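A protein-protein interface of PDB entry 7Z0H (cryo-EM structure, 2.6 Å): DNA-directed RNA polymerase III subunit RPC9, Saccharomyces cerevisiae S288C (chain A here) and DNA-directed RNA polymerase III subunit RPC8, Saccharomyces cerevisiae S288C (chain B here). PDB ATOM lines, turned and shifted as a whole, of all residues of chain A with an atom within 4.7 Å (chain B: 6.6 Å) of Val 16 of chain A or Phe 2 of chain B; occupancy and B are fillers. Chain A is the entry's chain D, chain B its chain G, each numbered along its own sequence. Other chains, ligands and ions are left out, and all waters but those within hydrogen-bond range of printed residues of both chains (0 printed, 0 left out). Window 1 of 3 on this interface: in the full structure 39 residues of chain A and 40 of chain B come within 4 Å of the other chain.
Hydrophobic or aromatic side chains of chain A that line the printed part of chain B: Phe 10, Leu 11, Val 16, Phe 19 and Val 62. Among the printed residues, no Asp or Glu carboxylate lies within 4 Å of a Lys or Arg side-chain nitrogen of the other chain.
The backbone carbonyl oxygen of Ile 3 of chain B sits at hydrogen-bond distance from the backbone NH of Val 76 of chain B, at 2.8 Å.
The backbone NH (N) of Leu 11 of chain A sits close to the backbone carbonyl oxygen (O) of Phe 2 of chain B (3.3 Å).
Of chain B, only Phe 2 (3.6 Å) comes within 4 Å of Val 16 of chain A. Phe 2 of chain B touches just these residues of chain A: Leu 11 (3.2 Å), Asp 13 (3.96 Å), Val 16 (3.6 Å) and Val 62 (3.5 Å). Of the printed residues of chain B, Phe 19 of chain A touches Tyr 49 (3.5 Å). Printed residues of chain A within 4 Å of Leu 4 of chain B: Leu 11 (3.4 Å). Of the printed residues of chain A, Ile 3 of chain B touches Phe 10 and Leu 11. Of the printed residues of chain B, Leu 11 of chain A touches Phe 2 (3.2 Å), Ile 3 (3.8 Å) and Leu 4 (3.4 Å). Pro 79 of chain B touches none of the printed residues of chain A. The nearest residue of chain A that does not touch Phe 2 of chain B is Phe 10 of chain A (4.3 Å). The nearest printed residue of chain B that does not touch Phe 10 of chain A is Phe 2 of chain B (4.3 Å).
Among the printed residues, pairs that only touch across the chains: Phe 10 of chain A with Ile 3 of chain B, Leu 11 of chain A with Ile 3 of chain B, Leu 11 of chain A with Leu 4 of chain B, Asp 13 of chain A with Phe 2 of chain B, Val 16 of chain A with Phe 2 of chain B, Phe 19 of chain A with Tyr 49 of chain B, Val 62 of chain A with Phe 2 of chain B and Val 62 of chain A with Ile 104 of chain B.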
ATOM      1  N   PHE A  10     -23.144   1.503   8.454  1.00  0.00           N
ATOM      2  CA  PHE A  10     -22.395   2.263   9.436  1.00  0.00           C
ATOM      3  C   PHE A  10     -20.917   2.311   9.055  1.00  0.00           C
ATOM      4  O   PHE A  10     -20.464   1.658   8.110  1.00  0.00           O
ATOM      5  CB  PHE A  10     -22.558   1.649  10.825  1.00  0.00           C
ATOM      6  CG  PHE A  10     -23.930   1.820  11.407  1.00  0.00           C
ATOM      7  CD1 PHE A  10     -24.356   3.055  11.865  1.00  0.00           C
ATOM      8  CD2 PHE A  10     -24.794   0.742  11.498  1.00  0.00           C
ATOM      9  CE1 PHE A  10     -25.618   3.211  12.404  1.00  0.00           C
ATOM     10  CE2 PHE A  10     -26.056   0.891  12.034  1.00  0.00           C
ATOM     11  CZ  PHE A  10     -26.469   2.127  12.486  1.00  0.00           C
ATOM     12  N   LEU A  11     -20.160   3.106   9.805  1.00  0.00           N
ATOM     13  CA  LEU A  11     -18.713   3.183   9.657  1.00  0.00           C
ATOM     14  C   LEU A  11     -18.055   2.830  10.981  1.00  0.00           C
ATOM     15  O   LEU A  11     -18.443   3.354  12.031  1.00  0.00           O
ATOM     16  CB  LEU A  11     -18.259   4.579   9.214  1.00  0.00           C
ATOM     17  CG  LEU A  11     -18.224   4.892   7.717  1.00  0.00           C
ATOM     18  CD1 LEU A  11     -17.327   3.908   6.978  1.00  0.00           C
ATOM     19  CD2 LEU A  11     -19.619   4.902   7.133  1.00  0.00           C
ATOM     20  N   SER A  12     -17.071   1.939  10.928  1.00  0.00           N
ATOM     21  CA  SER A  12     -16.179   1.759  12.062  1.00  0.00           C
ATOM     22  C   SER A  12     -15.174   2.899  12.084  1.00  0.00           C
ATOM     23  O   SER A  12     -14.643   3.295  11.043  1.00  0.00           O
ATOM     24  CB  SER A  12     -15.456   0.417  11.975  1.00  0.00           C
ATOM     25  OG  SER A  12     -15.146   0.091  10.632  1.00  0.00           O
ATOM     26  N   ASP A  13     -14.905   3.433  13.273  1.00  0.00           N
ATOM     27  CA  ASP A  13     -14.054   4.612  13.338  1.00  0.00           C
ATOM     28  C   ASP A  13     -12.582   4.226  13.266  1.00  0.00           C
ATOM     29  O   ASP A  13     -11.762   4.682  14.069  1.00  0.00           O
ATOM     30  CB  ASP A  13     -14.359   5.416  14.603  1.00  0.00           C
ATOM     31  CG  ASP A  13     -15.718   6.092  14.544  1.00  0.00           C
ATOM     32  OD1 ASP A  13     -16.217   6.318  13.423  1.00  0.00           O
ATOM     33  OD2 ASP A  13     -16.291   6.389  15.612  1.00  0.00           O
ATOM     34  N   TYR A  14     -12.255   3.373  12.297  1.00  0.00           N
ATOM     35  CA  TYR A  14     -10.914   3.238  11.746  1.00  0.00           C
ATOM     36  C   TYR A  14     -11.038   3.272  10.230  1.00  0.00           C
ATOM     37  O   TYR A  14     -10.132   3.731   9.530  1.00  0.00           O
ATOM     38  CB  TYR A  14     -10.235   1.944  12.195  1.00  0.00           C
ATOM     39  CG  TYR A  14      -8.997   1.621  11.385  1.00  0.00           C
ATOM     40  CD1 TYR A  14      -7.949   2.530  11.288  1.00  0.00           C
ATOM     41  CD2 TYR A  14      -8.892   0.427  10.686  1.00  0.00           C
ATOM     42  CE1 TYR A  14      -6.823   2.247  10.536  1.00  0.00           C
ATOM     43  CE2 TYR A  14      -7.769   0.136   9.931  1.00  0.00           C
ATOM     44  CZ  TYR A  14      -6.739   1.050   9.861  1.00  0.00           C
ATOM     45  OH  TYR A  14      -5.620   0.766   9.112  1.00  0.00           O
ATOM     46  N   GLU A  15     -12.172   2.780   9.721  1.00  0.00           N
ATOM     47  CA  GLU A  15     -12.421   2.821   8.284  1.00  0.00           C
ATOM     48  C   GLU A  15     -12.466   4.257   7.782  1.00  0.00           C
ATOM     49  O   GLU A  15     -11.887   4.577   6.739  1.00  0.00           O
ATOM     50  CB  GLU A  15     -13.724   2.091   7.957  1.00  0.00           C
ATOM     51  CG  GLU A  15     -13.575   0.582   7.826  1.00  0.00           C
ATOM     52  CD  GLU A  15     -14.794  -0.077   7.207  1.00  0.00           C
ATOM     53  OE1 GLU A  15     -15.606   0.637   6.582  1.00  0.00           O
ATOM     54  OE2 GLU A  15     -14.940  -1.310   7.348  1.00  0.00           O
ATOM     55  N   VAL A  16     -13.130   5.143   8.527  1.00  0.00           N
ATOM     56  CA  VAL A  16     -13.142   6.555   8.163  1.00  0.00           C
ATOM     57  C   VAL A  16     -11.745   7.153   8.285  1.00  0.00           C
ATOM     58  O   VAL A  16     -11.355   8.009   7.481  1.00  0.00           O
ATOM     59  CB  VAL A  16     -14.173   7.316   9.023  1.00  0.00           C
ATOM     60  CG1 VAL A  16     -13.947   7.041  10.502  1.00  0.00           C
ATOM     61  CG2 VAL A  16     -14.121   8.808   8.734  1.00  0.00           C
ATOM     62  N   LEU A  17     -10.967   6.710   9.275  1.00  0.00           N
ATOM     63  CA  LEU A  17      -9.608   7.219   9.428  1.00  0.00           C
ATOM     64  C   LEU A  17      -8.754   6.866   8.216  1.00  0.00           C
ATOM     65  O   LEU A  17      -8.067   7.728   7.658  1.00  0.00           O
ATOM     66  CB  LEU A  17      -8.983   6.673  10.715  1.00  0.00           C
ATOM     67  CG  LEU A  17      -7.731   7.362  11.277  1.00  0.00           C
ATOM     68  CD1 LEU A  17      -6.453   7.004  10.519  1.00  0.00           C
ATOM     69  CD2 LEU A  17      -7.930   8.870  11.299  1.00  0.00           C
ATOM     70  N   LYS A  18      -8.786   5.600   7.794  1.00  0.00           N
ATOM     71  CA  LYS A  18      -7.999   5.213   6.628  1.00  0.00           C
ATOM     72  C   LYS A  18      -8.562   5.823   5.353  1.00  0.00           C
ATOM     73  O   LYS A  18      -7.806   6.088   4.416  1.00  0.00           O
ATOM     74  CB  LYS A  18      -7.914   3.691   6.498  1.00  0.00           C
ATOM     75  CG  LYS A  18      -9.241   2.963   6.523  1.00  0.00           C
ATOM     76  CD  LYS A  18      -9.201   1.731   5.632  1.00  0.00           C
ATOM     77  CE  LYS A  18     -10.249   0.709   6.039  1.00  0.00           C
ATOM     78  NZ  LYS A  18      -9.763  -0.686   5.852  1.00  0.00           N
ATOM     79  N   PHE A  19      -9.872   6.077   5.300  1.00  0.00           N
ATOM     80  CA  PHE A  19     -10.445   6.757   4.143  1.00  0.00           C
ATOM     81  C   PHE A  19      -9.921   8.184   4.023  1.00  0.00           C
ATOM     82  O   PHE A  19      -9.531   8.625   2.937  1.00  0.00           O
ATOM     83  CB  PHE A  19     -11.970   6.746   4.233  1.00  0.00           C
ATOM     84  CG  PHE A  19     -12.650   7.403   3.069  1.00  0.00           C
ATOM     85  CD1 PHE A  19     -12.165   7.238   1.782  1.00  0.00           C
ATOM     86  CD2 PHE A  19     -13.769   8.195   3.261  1.00  0.00           C
ATOM     87  CE1 PHE A  19     -12.787   7.845   0.709  1.00  0.00           C
ATOM     88  CE2 PHE A  19     -14.395   8.804   2.192  1.00  0.00           C
ATOM     89  CZ  PHE A  19     -13.903   8.629   0.915  1.00  0.00           C
ATOM     90  N   LEU A  20      -9.898   8.923   5.135  1.00  0.00           N
ATOM     91  CA  LEU A  20      -9.376  10.288   5.096  1.00  0.00           C
ATOM     92  C   LEU A  20      -7.870  10.293   4.857  1.00  0.00           C
ATOM     93  O   LEU A  20      -7.342  11.181   4.174  1.00  0.00           O
ATOM     94  CB  LEU A  20      -9.726  11.021   6.389  1.00  0.00           C
ATOM     95  CG  LEU A  20     -10.999  11.868   6.325  1.00  0.00           C
ATOM     96  CD1 LEU A  20     -12.224  11.008   6.562  1.00  0.00           C
ATOM     97  CD2 LEU A  20     -10.946  13.002   7.333  1.00  0.00           C
ATOM     98  N   VAL A  62     -11.573  16.471  11.013  1.00  0.00           N
ATOM     99  CA  VAL A  62     -11.893  15.135  11.510  1.00  0.00           C
ATOM    100  C   VAL A  62     -10.621  14.345  11.784  1.00  0.00           C
ATOM    101  O   VAL A  62     -10.504  13.664  12.812  1.00  0.00           O
ATOM    102  CB  VAL A  62     -12.811  14.401  10.514  1.00  0.00           C
ATOM    103  CG1 VAL A  62     -12.827  12.911  10.807  1.00  0.00           C
ATOM    104  CG2 VAL A  62     -14.218  14.972  10.572  1.00  0.00           C
ATOM    105  N   PHE B   2     -20.265   8.700  12.465  1.00  0.00           N
ATOM    106  CA  PHE B   2     -19.960   8.579  11.045  1.00  0.00           C
ATOM    107  C   PHE B   2     -20.762   7.450  10.408  1.00  0.00           C
ATOM    108  O   PHE B   2     -20.546   6.278  10.710  1.00  0.00           O
ATOM    109  CB  PHE B   2     -18.463   8.342  10.836  1.00  0.00           C
ATOM    110  CG  PHE B   2     -17.658   9.604  10.754  1.00  0.00           C
ATOM    111  CD1 PHE B   2     -18.142  10.706  10.070  1.00  0.00           C
ATOM    112  CD2 PHE B   2     -16.418   9.691  11.362  1.00  0.00           C
ATOM    113  CE1 PHE B   2     -17.405  11.870   9.992  1.00  0.00           C
ATOM    114  CE2 PHE B   2     -15.677  10.852  11.288  1.00  0.00           C
ATOM    115  CZ  PHE B   2     -16.172  11.943  10.602  1.00  0.00           C
ATOM    116  N   ILE B   3     -21.691   7.812   9.528  1.00  0.00           N
ATOM    117  CA  ILE B   3     -22.535   6.843   8.840  1.00  0.00           C
ATOM    118  C   ILE B   3     -22.627   7.231   7.370  1.00  0.00           C
ATOM    119  O   ILE B   3     -22.666   8.418   7.029  1.00  0.00           O
ATOM    120  CB  ILE B   3     -23.938   6.752   9.480  1.00  0.00           C
ATOM    121  CG1 ILE B   3     -24.772   5.662   8.804  1.00  0.00           C
ATOM    122  CG2 ILE B   3     -24.650   8.094   9.419  1.00  0.00           C
ATOM    123  CD1 ILE B   3     -26.126   5.451   9.440  1.00  0.00           C
ATOM    124  N   LEU B   4     -22.637   6.226   6.499  1.00  0.00           N
ATOM    125  CA  LEU B   4     -22.833   6.465   5.079  1.00  0.00           C
ATOM    126  C   LEU B   4     -24.282   6.857   4.796  1.00  0.00           C
ATOM    127  O   LEU B   4     -25.171   6.737   5.645  1.00  0.00           O
ATOM    128  CB  LEU B   4     -22.462   5.223   4.267  1.00  0.00           C
ATOM    129  CG  LEU B   4     -20.997   5.012   3.892  1.00  0.00           C
ATOM    130  CD1 LEU B   4     -20.871   3.975   2.788  1.00  0.00           C
ATOM    131  CD2 LEU B   4     -20.361   6.323   3.467  1.00  0.00           C
ATOM    132  N   LEU B  44     -24.562  16.497   8.249  1.00  0.00           N
ATOM    133  CA  LEU B  44     -23.424  17.251   7.742  1.00  0.00           C
ATOM    134  C   LEU B  44     -22.571  16.344   6.867  1.00  0.00           C
ATOM    135  O   LEU B  44     -22.249  15.219   7.263  1.00  0.00           O
ATOM    136  CB  LEU B  44     -22.586  17.817   8.890  1.00  0.00           C
ATOM    137  CG  LEU B  44     -21.159  18.247   8.547  1.00  0.00           C
ATOM    138  CD1 LEU B  44     -21.125  19.668   8.010  1.00  0.00           C
ATOM    139  CD2 LEU B  44     -20.251  18.105   9.758  1.00  0.00           C
ATOM    140  N   ILE B  46     -19.139  15.318   5.077  1.00  0.00           N
ATOM    141  CA  ILE B  46     -17.689  15.462   5.122  1.00  0.00           C
ATOM    142  C   ILE B  46     -17.086  15.355   3.729  1.00  0.00           C
ATOM    143  O   ILE B  46     -16.333  16.232   3.297  1.00  0.00           O
ATOM    144  CB  ILE B  46     -17.078  14.415   6.077  1.00  0.00           C
ATOM    145  CG1 ILE B  46     -17.901  14.304   7.364  1.00  0.00           C
ATOM    146  CG2 ILE B  46     -15.633  14.765   6.395  1.00  0.00           C
ATOM    147  CD1 ILE B  46     -18.032  15.607   8.127  1.00  0.00           C
ATOM    148  N   TYR B  49     -17.892   9.040  -0.367  1.00  0.00           N
ATOM    149  CA  TYR B  49     -17.190   7.774  -0.185  1.00  0.00           C
ATOM    150  C   TYR B  49     -16.777   7.177  -1.525  1.00  0.00           C
ATOM    151  O   TYR B  49     -15.584   7.001  -1.800  1.00  0.00           O
ATOM    152  CB  TYR B  49     -18.072   6.798   0.597  1.00  0.00           C
ATOM    153  CG  TYR B  49     -17.316   5.673   1.260  1.00  0.00           C
ATOM    154  CD1 TYR B  49     -16.310   5.934   2.180  1.00  0.00           C
ATOM    155  CD2 TYR B  49     -17.609   4.350   0.968  1.00  0.00           C
ATOM    156  CE1 TYR B  49     -15.616   4.906   2.789  1.00  0.00           C
ATOM    157  CE2 TYR B  49     -16.921   3.316   1.572  1.00  0.00           C
ATOM    158  CZ  TYR B  49     -15.926   3.600   2.481  1.00  0.00           C
ATOM    159  OH  TYR B  49     -15.240   2.571   3.084  1.00  0.00           O
ATOM    160  N   VAL B  75     -20.242  10.279   3.403  1.00  0.00           N
ATOM    161  CA  VAL B  75     -20.078  10.152   4.847  1.00  0.00           C
ATOM    162  C   VAL B  75     -20.788  11.314   5.535  1.00  0.00           C
ATOM    163  O   VAL B  75     -20.475  12.484   5.294  1.00  0.00           O
ATOM    164  CB  VAL B  75     -18.593  10.092   5.232  1.00  0.00           C
ATOM    165  CG1 VAL B  75     -18.018   8.733   4.884  1.00  0.00           C
ATOM    166  CG2 VAL B  75     -17.807  11.175   4.513  1.00  0.00           C
ATOM    167  N   VAL B  76     -21.760  10.988   6.384  1.00  0.00           N
ATOM    168  CA  VAL B  76     -22.549  11.972   7.114  1.00  0.00           C
ATOM    169  C   VAL B  76     -22.394  11.704   8.604  1.00  0.00           C
ATOM    170  O   VAL B  76     -22.499  10.555   9.047  1.00  0.00           O
ATOM    171  CB  VAL B  76     -24.034  11.935   6.703  1.00  0.00           C
ATOM    172  CG1 VAL B  76     -24.759  13.157   7.232  1.00  0.00           C
ATOM    173  CG2 VAL B  76     -24.165  11.856   5.191  1.00  0.00           C
ATOM    174  N   PHE B  77     -22.141  12.762   9.371  1.00  0.00           N
ATOM    175  CA  PHE B  77     -21.934  12.659  10.814  1.00  0.00           C
ATOM    176  C   PHE B  77     -23.299  12.685  11.492  1.00  0.00           C
ATOM    177  O   PHE B  77     -23.903  13.746  11.662  1.00  0.00           O
ATOM    178  CB  PHE B  77     -21.035  13.794  11.294  1.00  0.00           C
ATOM    179  CG  PHE B  77     -20.878  13.867  12.786  1.00  0.00           C
ATOM    180  CD1 PHE B  77     -19.905  13.120  13.426  1.00  0.00           C
ATOM    181  CD2 PHE B  77     -21.678  14.706  13.544  1.00  0.00           C
ATOM    182  CE1 PHE B  77     -19.748  13.188  14.796  1.00  0.00           C
ATOM    183  CE2 PHE B  77     -21.524  14.778  14.915  1.00  0.00           C
ATOM    184  CZ  PHE B  77     -20.558  14.019  15.542  1.00  0.00           C
ATOM    185  N   LYS B  78     -23.801  11.508  11.874  1.00  0.00           N
ATOM    186  CA  LYS B  78     -25.159  11.364  12.400  1.00  0.00           C
ATOM    187  C   LYS B  78     -25.211  10.541  13.681  1.00  0.00           C
ATOM    188  O   LYS B  78     -25.569   9.356  13.656  1.00  0.00           O
ATOM    189  CB  LYS B  78     -26.079  10.747  11.349  1.00  0.00           C
ATOM    190  CG  LYS B  78     -26.954  11.758  10.654  1.00  0.00           C
ATOM    191  CD  LYS B  78     -27.708  12.573  11.682  1.00  0.00           C
ATOM    192  CE  LYS B  78     -28.723  13.472  11.027  1.00  0.00           C
ATOM    193  NZ  LYS B  78     -28.315  14.887  11.181  1.00  0.00           N
ATOM    194  N   PRO B  79     -24.860  11.134  14.825  1.00  0.00           N
ATOM    195  CA  PRO B  79     -25.179  10.499  16.113  1.00  0.00           C
ATOM    196  C   PRO B  79     -26.691  10.397  16.281  1.00  0.00           C
ATOM    197  O   PRO B  79     -27.428  11.290  15.857  1.00  0.00           O
ATOM    198  CB  PRO B  79     -24.567  11.450  17.146  1.00  0.00           C
ATOM    199  CG  PRO B  79     -23.550  12.235  16.407  1.00  0.00           C
ATOM    200  CD  PRO B  79     -23.985  12.307  14.977  1.00  0.00           C
ATOM    201  N   ILE B 104     -15.353  21.898  13.041  1.00  0.00           N
ATOM    202  CA  ILE B 104     -16.228  21.055  12.233  1.00  0.00           C
ATOM    203  C   ILE B 104     -17.615  21.681  12.191  1.00  0.00           C
ATOM    204  O   ILE B 104     -18.097  22.087  11.129  1.00  0.00           O
ATOM    205  CB  ILE B 104     -16.295  19.621  12.790  1.00  0.00           C
ATOM    206  CG1 ILE B 104     -14.908  18.982  12.800  1.00  0.00           C
ATOM    207  CG2 ILE B 104     -17.250  18.776  11.964  1.00  0.00           C
ATOM    208  CD1 ILE B 104     -14.907  17.521  13.188  1.00  0.00           C
